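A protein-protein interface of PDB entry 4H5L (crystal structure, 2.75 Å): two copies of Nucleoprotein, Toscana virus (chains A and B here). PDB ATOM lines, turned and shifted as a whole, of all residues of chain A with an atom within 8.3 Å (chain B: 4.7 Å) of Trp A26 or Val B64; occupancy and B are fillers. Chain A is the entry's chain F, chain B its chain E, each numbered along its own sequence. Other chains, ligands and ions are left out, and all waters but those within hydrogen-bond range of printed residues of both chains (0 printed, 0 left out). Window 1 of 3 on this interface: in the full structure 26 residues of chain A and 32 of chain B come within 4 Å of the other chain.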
ATOM      1  N   SER A  17      -0.451 -15.820  14.217  1.00  0.00           N
ATOM      2  CA  SER A  17       0.406 -14.726  13.740  1.00  0.00           C
ATOM      3  C   SER A  17      -0.348 -13.453  13.365  1.00  0.00           C
ATOM      4  O   SER A  17      -1.381 -13.501  12.702  1.00  0.00           O
ATOM      5  CB  SER A  17       1.237 -15.176  12.541  1.00  0.00           C
ATOM      6  OG  SER A  17       0.438 -15.466  11.407  1.00  0.00           O
ATOM      7  N   ALA A  18       0.206 -12.312  13.775  1.00  0.00           N
ATOM      8  CA  ALA A  18      -0.323 -10.987  13.469  1.00  0.00           C
ATOM      9  C   ALA A  18       0.855 -10.089  13.036  1.00  0.00           C
ATOM     10  O   ALA A  18       1.248  -9.168  13.754  1.00  0.00           O
ATOM     11  CB  ALA A  18      -1.068 -10.420  14.671  1.00  0.00           C
ATOM     12  N   ASP A  19       1.442 -10.406  11.861  1.00  0.00           N
ATOM     13  CA  ASP A  19       2.601  -9.706  11.287  1.00  0.00           C
ATOM     14  C   ASP A  19       2.225  -8.308  10.801  1.00  0.00           C
ATOM     15  O   ASP A  19       1.502  -8.176   9.813  1.00  0.00           O
ATOM     16  CB  ASP A  19       3.238 -10.507  10.125  1.00  0.00           C
ATOM     17  CG  ASP A  19       3.030 -12.018  10.164  1.00  0.00           C
ATOM     18  OD1 ASP A  19       3.584 -12.665  11.063  1.00  0.00           O
ATOM     19  OD2 ASP A  19       2.334 -12.553   9.265  1.00  0.00           O
ATOM     20  N   SER A  20       2.749  -7.266  11.475  1.00  0.00           N
ATOM     21  CA  SER A  20       2.513  -5.851  11.154  1.00  0.00           C
ATOM     22  C   SER A  20       2.820  -5.521   9.685  1.00  0.00           C
ATOM     23  O   SER A  20       2.194  -4.628   9.120  1.00  0.00           O
ATOM     24  CB  SER A  20       3.347  -4.951  12.061  1.00  0.00           C
ATOM     25  OG  SER A  20       4.736  -5.164  11.865  1.00  0.00           O
ATOM     26  N   GLY A  21       3.764  -6.254   9.094  1.00  0.00           N
ATOM     27  CA  GLY A  21       4.163  -6.095   7.702  1.00  0.00           C
ATOM     28  C   GLY A  21       3.072  -6.486   6.728  1.00  0.00           C
ATOM     29  O   GLY A  21       2.662  -5.666   5.903  1.00  0.00           O
ATOM     30  N   THR A  22       2.579  -7.735   6.838  1.00  0.00           N
ATOM     31  CA  THR A  22       1.523  -8.282   5.975  1.00  0.00           C
ATOM     32  C   THR A  22       0.151  -7.647   6.286  1.00  0.00           C
ATOM     33  O   THR A  22      -0.718  -7.634   5.413  1.00  0.00           O
ATOM     34  CB  THR A  22       1.459  -9.812   6.077  1.00  0.00           C
ATOM     35  OG1 THR A  22       1.253 -10.175   7.435  1.00  0.00           O
ATOM     36  CG2 THR A  22       2.722 -10.500   5.554  1.00  0.00           C
ATOM     37  N   ILE A  23      -0.040  -7.117   7.514  1.00  0.00           N
ATOM     38  CA  ILE A  23      -1.287  -6.455   7.904  1.00  0.00           C
ATOM     39  C   ILE A  23      -1.326  -5.074   7.230  1.00  0.00           C
ATOM     40  O   ILE A  23      -2.328  -4.754   6.598  1.00  0.00           O
ATOM     41  CB  ILE A  23      -1.498  -6.401   9.444  1.00  0.00           C
ATOM     42  CG1 ILE A  23      -1.835  -7.820   9.989  1.00  0.00           C
ATOM     43  CG2 ILE A  23      -2.613  -5.413   9.809  1.00  0.00           C
ATOM     44  CD1 ILE A  23      -1.785  -8.015  11.516  1.00  0.00           C
ATOM     45  N   ASN A  24      -0.227  -4.291   7.310  1.00  0.00           N
ATOM     46  CA  ASN A  24      -0.131  -2.974   6.669  1.00  0.00           C
ATOM     47  C   ASN A  24      -0.166  -3.099   5.149  1.00  0.00           C
ATOM     48  O   ASN A  24      -0.619  -2.173   4.480  1.00  0.00           O
ATOM     49  CB  ASN A  24       1.110  -2.211   7.120  1.00  0.00           C
ATOM     50  CG  ASN A  24       1.021  -1.702   8.544  1.00  0.00           C
ATOM     51  OD1 ASN A  24      -0.060  -1.358   9.057  1.00  0.00           O
ATOM     52  ND2 ASN A  24       2.165  -1.633   9.216  1.00  0.00           N
ATOM     53  N   ALA A  25       0.261  -4.258   4.613  1.00  0.00           N
ATOM     54  CA  ALA A  25       0.205  -4.560   3.190  1.00  0.00           C
ATOM     55  C   ALA A  25      -1.258  -4.729   2.765  1.00  0.00           C
ATOM     56  O   ALA A  25      -1.652  -4.255   1.691  1.00  0.00           O
ATOM     57  CB  ALA A  25       1.000  -5.820   2.895  1.00  0.00           C
ATOM     58  N   TRP A  26      -2.069  -5.370   3.639  1.00  0.00           N
ATOM     59  CA  TRP A  26      -3.500  -5.571   3.429  1.00  0.00           C
ATOM     60  C   TRP A  26      -4.251  -4.250   3.580  1.00  0.00           C
ATOM     61  O   TRP A  26      -5.127  -3.968   2.766  1.00  0.00           O
ATOM     62  CB  TRP A  26      -4.066  -6.608   4.414  1.00  0.00           C
ATOM     63  CG  TRP A  26      -3.618  -8.022   4.200  1.00  0.00           C
ATOM     64  CD1 TRP A  26      -3.090  -8.560   3.066  1.00  0.00           C
ATOM     65  CD2 TRP A  26      -3.731  -9.097   5.139  1.00  0.00           C
ATOM     66  NE1 TRP A  26      -2.837  -9.898   3.249  1.00  0.00           N
ATOM     67  CE2 TRP A  26      -3.215 -10.254   4.516  1.00  0.00           C
ATOM     68  CE3 TRP A  26      -4.206  -9.192   6.458  1.00  0.00           C
ATOM     69  CZ2 TRP A  26      -3.163 -11.495   5.165  1.00  0.00           C
ATOM     70  CZ3 TRP A  26      -4.160 -10.419   7.095  1.00  0.00           C
ATOM     71  CH2 TRP A  26      -3.651 -11.555   6.449  1.00  0.00           C
ATOM     72  N   VAL A  27      -3.904  -3.442   4.617  1.00  0.00           N
ATOM     73  CA  VAL A  27      -4.504  -2.133   4.918  1.00  0.00           C
ATOM     74  C   VAL A  27      -4.407  -1.241   3.676  1.00  0.00           C
ATOM     75  O   VAL A  27      -5.422  -0.691   3.259  1.00  0.00           O
ATOM     76  CB  VAL A  27      -3.859  -1.469   6.165  1.00  0.00           C
ATOM     77  CG1 VAL A  27      -4.204   0.014   6.260  1.00  0.00           C
ATOM     78  CG2 VAL A  27      -4.276  -2.188   7.437  1.00  0.00           C
ATOM     79  N   ASN A  28      -3.206  -1.160   3.061  1.00  0.00           N
ATOM     80  CA  ASN A  28      -2.935  -0.372   1.860  1.00  0.00           C
ATOM     81  C   ASN A  28      -3.739  -0.881   0.674  1.00  0.00           C
ATOM     82  O   ASN A  28      -4.286  -0.072  -0.073  1.00  0.00           O
ATOM     83  CB  ASN A  28      -1.436  -0.382   1.536  1.00  0.00           C
ATOM     84  CG  ASN A  28      -0.575   0.447   2.478  1.00  0.00           C
ATOM     85  OD1 ASN A  28      -1.026   1.402   3.143  1.00  0.00           O
ATOM     86  ND2 ASN A  28       0.707   0.116   2.530  1.00  0.00           N
ATOM     87  N   GLU A  29      -3.842  -2.210   0.522  1.00  0.00           N
ATOM     88  CA  GLU A  29      -4.587  -2.826  -0.576  1.00  0.00           C
ATOM     89  C   GLU A  29      -6.116  -2.701  -0.396  1.00  0.00           C
ATOM     90  O   GLU A  29      -6.840  -2.670  -1.391  1.00  0.00           O
ATOM     91  CB  GLU A  29      -4.188  -4.298  -0.733  1.00  0.00           C
ATOM     92  CG  GLU A  29      -4.341  -4.831  -2.150  1.00  0.00           C
ATOM     93  CD  GLU A  29      -3.447  -4.198  -3.209  1.00  0.00           C
ATOM     94  OE1 GLU A  29      -2.252  -4.574  -3.277  1.00  0.00           O
ATOM     95  OE2 GLU A  29      -3.940  -3.331  -3.971  1.00  0.00           O
ATOM     96  N   PHE A  30      -6.602  -2.608   0.857  1.00  0.00           N
ATOM     97  CA  PHE A  30      -8.033  -2.507   1.163  1.00  0.00           C
ATOM     98  C   PHE A  30      -8.537  -1.067   1.375  1.00  0.00           C
ATOM     99  O   PHE A  30      -9.746  -0.852   1.259  1.00  0.00           O
ATOM    100  CB  PHE A  30      -8.383  -3.344   2.412  1.00  0.00           C
ATOM    101  CG  PHE A  30      -8.264  -4.844   2.284  1.00  0.00           C
ATOM    102  CD1 PHE A  30      -8.614  -5.491   1.102  1.00  0.00           C
ATOM    103  CD2 PHE A  30      -7.877  -5.619   3.368  1.00  0.00           C
ATOM    104  CE1 PHE A  30      -8.532  -6.882   0.997  1.00  0.00           C
ATOM    105  CE2 PHE A  30      -7.796  -7.010   3.262  1.00  0.00           C
ATOM    106  CZ  PHE A  30      -8.120  -7.633   2.076  1.00  0.00           C
ATOM    107  N   ALA A  31      -7.627  -0.098   1.673  1.00  0.00           N
ATOM    108  CA  ALA A  31      -7.917   1.322   1.961  1.00  0.00           C
ATOM    109  C   ALA A  31      -8.825   2.005   0.931  1.00  0.00           C
ATOM    110  O   ALA A  31      -8.876   1.585  -0.231  1.00  0.00           O
ATOM    111  CB  ALA A  31      -6.620   2.108   2.074  1.00  0.00           C
ATOM    112  N   LYS B  57      -6.277 -17.643   7.540  1.00  0.00           N
ATOM    113  CA  LYS B  57      -5.697 -16.453   6.913  1.00  0.00           C
ATOM    114  C   LYS B  57      -6.838 -15.535   6.495  1.00  0.00           C
ATOM    115  O   LYS B  57      -6.741 -14.323   6.670  1.00  0.00           O
ATOM    116  CB  LYS B  57      -4.811 -16.831   5.701  1.00  0.00           C
ATOM    117  CG  LYS B  57      -3.812 -15.742   5.287  1.00  0.00           C
ATOM    118  CD  LYS B  57      -3.039 -16.066   4.001  1.00  0.00           C
ATOM    119  CE  LYS B  57      -3.711 -15.499   2.763  1.00  0.00           C
ATOM    120  NZ  LYS B  57      -2.785 -15.422   1.593  1.00  0.00           N
ATOM    121  N   LYS B  60      -8.384 -13.428   9.299  1.00  0.00           N
ATOM    122  CA  LYS B  60      -7.471 -12.335   9.575  1.00  0.00           C
ATOM    123  C   LYS B  60      -7.691 -11.210   8.582  1.00  0.00           C
ATOM    124  O   LYS B  60      -7.727 -10.039   8.972  1.00  0.00           O
ATOM    125  CB  LYS B  60      -6.038 -12.813   9.509  1.00  0.00           C
ATOM    126  CG  LYS B  60      -5.701 -13.705  10.637  1.00  0.00           C
ATOM    127  CD  LYS B  60      -4.234 -14.018  10.579  1.00  0.00           C
ATOM    128  CE  LYS B  60      -3.883 -15.048  11.607  1.00  0.00           C
ATOM    129  NZ  LYS B  60      -2.556 -15.634  11.318  1.00  0.00           N
ATOM    130  N   MET B  61      -7.878 -11.577   7.294  1.00  0.00           N
ATOM    131  CA  MET B  61      -8.121 -10.639   6.196  1.00  0.00           C
ATOM    132  C   MET B  61      -9.473  -9.974   6.384  1.00  0.00           C
ATOM    133  O   MET B  61      -9.552  -8.747   6.306  1.00  0.00           O
ATOM    134  CB  MET B  61      -8.041 -11.333   4.828  1.00  0.00           C
ATOM    135  CG  MET B  61      -6.645 -11.759   4.452  1.00  0.00           C
ATOM    136  SD  MET B  61      -6.284 -11.752   2.678  1.00  0.00           S
ATOM    137  CE  MET B  61      -7.191 -13.218   2.153  1.00  0.00           C
ATOM    138  N   MET B  62     -10.518 -10.776   6.680  1.00  0.00           N
ATOM    139  CA  MET B  62     -11.878 -10.287   6.910  1.00  0.00           C
ATOM    140  C   MET B  62     -11.888  -9.310   8.111  1.00  0.00           C
ATOM    141  O   MET B  62     -12.538  -8.267   8.015  1.00  0.00           O
ATOM    142  CB  MET B  62     -12.873 -11.453   7.096  1.00  0.00           C
ATOM    143  CG  MET B  62     -13.228 -12.126   5.780  1.00  0.00           C
ATOM    144  SD  MET B  62     -14.495 -13.440   5.849  1.00  0.00           S
ATOM    145  CE  MET B  62     -13.556 -14.800   6.512  1.00  0.00           C
ATOM    146  N   ILE B  63     -11.110  -9.617   9.195  1.00  0.00           N
ATOM    147  CA  ILE B  63     -10.996  -8.740  10.365  1.00  0.00           C
ATOM    148  C   ILE B  63     -10.290  -7.418   9.941  1.00  0.00           C
ATOM    149  O   ILE B  63     -10.835  -6.339  10.190  1.00  0.00           O
ATOM    150  CB  ILE B  63     -10.306  -9.404  11.604  1.00  0.00           C
ATOM    151  CG1 ILE B  63     -11.163 -10.553  12.223  1.00  0.00           C
ATOM    152  CG2 ILE B  63      -9.988  -8.339  12.660  1.00  0.00           C
ATOM    153  CD1 ILE B  63     -10.492 -11.410  13.327  1.00  0.00           C
ATOM    154  N   VAL B  64      -9.127  -7.506   9.265  1.00  0.00           N
ATOM    155  CA  VAL B  64      -8.391  -6.327   8.788  1.00  0.00           C
ATOM    156  C   VAL B  64      -9.355  -5.463   7.954  1.00  0.00           C
ATOM    157  O   VAL B  64      -9.532  -4.283   8.270  1.00  0.00           O
ATOM    158  CB  VAL B  64      -7.085  -6.697   8.021  1.00  0.00           C
ATOM    159  CG1 VAL B  64      -6.626  -5.567   7.091  1.00  0.00           C
ATOM    160  CG2 VAL B  64      -5.969  -7.082   8.999  1.00  0.00           C
ATOM    161  N   LEU B  65     -10.048  -6.090   6.977  1.00  0.00           N
ATOM    162  CA  LEU B  65     -11.044  -5.473   6.104  1.00  0.00           C
ATOM    163  C   LEU B  65     -12.169  -4.780   6.916  1.00  0.00           C
ATOM    164  O   LEU B  65     -12.452  -3.622   6.640  1.00  0.00           O
ATOM    165  CB  LEU B  65     -11.614  -6.548   5.172  1.00  0.00           C
ATOM    166  CG  LEU B  65     -12.497  -6.098   4.020  1.00  0.00           C
ATOM    167  CD1 LEU B  65     -11.723  -5.256   3.023  1.00  0.00           C
ATOM    168  CD2 LEU B  65     -13.113  -7.294   3.326  1.00  0.00           C
ATOM    169  N   ASN B  66     -12.748  -5.449   7.945  1.00  0.00           N
ATOM    170  CA  ASN B  66     -13.804  -4.917   8.825  1.00  0.00           C
ATOM    171  C   ASN B  66     -13.321  -3.727   9.673  1.00  0.00           C
ATOM    172  O   ASN B  66     -14.102  -2.795   9.910  1.00  0.00           O
ATOM    173  CB  ASN B  66     -14.348  -6.018   9.772  1.00  0.00           C
ATOM    174  CG  ASN B  66     -15.503  -5.594  10.685  1.00  0.00           C
ATOM    175  OD1 ASN B  66     -15.437  -5.718  11.918  1.00  0.00           O
ATOM    176  ND2 ASN B  66     -16.608  -5.130  10.109  1.00  0.00           N
ATOM    177  N   LEU B  67     -12.085  -3.803  10.200  1.00  0.00           N
ATOM    178  CA  LEU B  67     -11.533  -2.750  11.053  1.00  0.00           C
ATOM    179  C   LEU B  67     -11.288  -1.452  10.294  1.00  0.00           C
ATOM    180  O   LEU B  67     -11.479  -0.366  10.852  1.00  0.00           O
ATOM    181  CB  LEU B  67     -10.207  -3.186  11.700  1.00  0.00           C
ATOM    182  CG  LEU B  67     -10.222  -4.375  12.667  1.00  0.00           C
ATOM    183  CD1 LEU B  67      -8.833  -4.954  12.819  1.00  0.00           C
ATOM    184  CD2 LEU B  67     -10.753  -3.992  14.005  1.00  0.00           C
ATOM    185  N   VAL B  68     -10.845  -1.566   9.030  1.00  0.00           N
ATOM    186  CA  VAL B  68     -10.447  -0.424   8.222  1.00  0.00           C
ATOM    187  C   VAL B  68     -11.551   0.029   7.206  1.00  0.00           C
ATOM    188  O   VAL B  68     -11.566   1.210   6.860  1.00  0.00           O
ATOM    189  CB  VAL B  68      -9.067  -0.728   7.548  1.00  0.00           C
ATOM    190  CG1 VAL B  68      -9.187  -1.668   6.351  1.00  0.00           C
ATOM    191  CG2 VAL B  68      -8.325   0.540   7.166  1.00  0.00           C
ATOM    192  N   TRP B 119      -8.028 -12.566  18.045  1.00  0.00           N
ATOM    193  CA  TRP B 119      -7.072 -12.135  17.025  1.00  0.00           C
ATOM    194  C   TRP B 119      -7.184 -10.633  16.737  1.00  0.00           C
ATOM    195  O   TRP B 119      -6.160  -9.946  16.688  1.00  0.00           O
ATOM    196  CB  TRP B 119      -7.184 -12.937  15.721  1.00  0.00           C
ATOM    197  CG  TRP B 119      -6.057 -12.614  14.784  1.00  0.00           C
ATOM    198  CD1 TRP B 119      -4.766 -13.058  14.869  1.00  0.00           C
ATOM    199  CD2 TRP B 119      -6.075 -11.633  13.729  1.00  0.00           C
ATOM    200  NE1 TRP B 119      -4.001 -12.484  13.875  1.00  0.00           N
ATOM    201  CE2 TRP B 119      -4.770 -11.569  13.190  1.00  0.00           C
ATOM    202  CE3 TRP B 119      -7.069 -10.799  13.186  1.00  0.00           C
ATOM    203  CZ2 TRP B 119      -4.452 -10.758  12.097  1.00  0.00           C
ATOM    204  CZ3 TRP B 119      -6.749  -9.993  12.095  1.00  0.00           C
ATOM    205  CH2 TRP B 119      -5.461  -9.994  11.554  1.00  0.00           C
ATOM    206  N   LEU B 127      -2.605  -1.530  13.364  1.00  0.00           N
ATOM    207  CA  LEU B 127      -3.281  -0.652  12.403  1.00  0.00           C
ATOM    208  C   LEU B 127      -4.139   0.427  13.092  1.00  0.00           C
ATOM    209  O   LEU B 127      -5.131   0.874  12.513  1.00  0.00           O
ATOM    210  CB  LEU B 127      -4.128  -1.452  11.376  1.00  0.00           C
ATOM    211  CG  LEU B 127      -4.950  -2.666  11.848  1.00  0.00           C
ATOM    212  CD1 LEU B 127      -6.157  -2.262  12.680  1.00  0.00           C
ATOM    213  CD2 LEU B 127      -5.470  -3.460  10.669  1.00  0.00           C
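NZ of Lys B60 is in hydrogen-bond range of O of Ser A17 (2.8 Å). O of Ser A17 sits at hydrogen-bond distance from NE1 of Trp B119 (3.0 Å).
Among the printed residues, pairs that only touch across the chains: Phe A30 with Leu B65 (3.6 Å), Trp A26 with Met B61 (3.6 Å), Ile A23 with Leu B127 (3.6 Å), Val A27 with Leu B127 (3.7 Å), Ala A18 with Trp B119 (3.7 Å), Trp A26 with Val B64 (3.7 Å), Ile A23 with Val B64 (3.8 Å), Ile A23 with Trp B119 (3.9 Å), Trp A26 with Lys B60 (3.9 Å), Phe A30 with Met B61 (3.9 Å) and Phe A30 with Val B64 (3.9 Å).
Trp A26 touches just these residues of chain B: Lys B60, Met B61 and Val B64. Of chain A, only Ile A23, Trp A26 and Phe A30 come within 4 Å of Val B64. Printed residues of chain B within 4 Å of Ser A17: Lys B60 and Trp B119. Of the printed residues of chain A, Lys B60 touches Ser A17 (2.8 Å) and Trp A26 (3.9 Å). Gly A21 touches none of the printed residues of chain B. The nearest residue of chain B that does not touch Trp A26 is Lys B57 (4.2 Å).
Of the 15 printed residues of chain A, 6 touch a printed residue of chain B. Hydrophobic or aromatic side chains of chain A that line the printed part of chain B: Ala A18, Ile A23, Trp A26, Val A27 and Phe A30. Of the 12 printed residues of chain B, 6 touch a printed residue of chain A. Printed residues of chain B that touch a printed residue of chain A: Lys B60, Met B61, Val B64, Leu B65, Trp B119 and Leu B127. Hydrophobic or aromatic side chains of chain B that line the printed part of chain A: Met B61, Val B64, Leu B65, Trp B119 and Leu B127. Among the printed residues, no Asp or Glu carboxylate lies within 4 Å of a Lys or Arg side-chain nitrogen of the other chain.
No position is printed for both chains. Of the 13 pairs that touch across the chains among the printed residues, none has its exchanged pair printed and touching as well.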
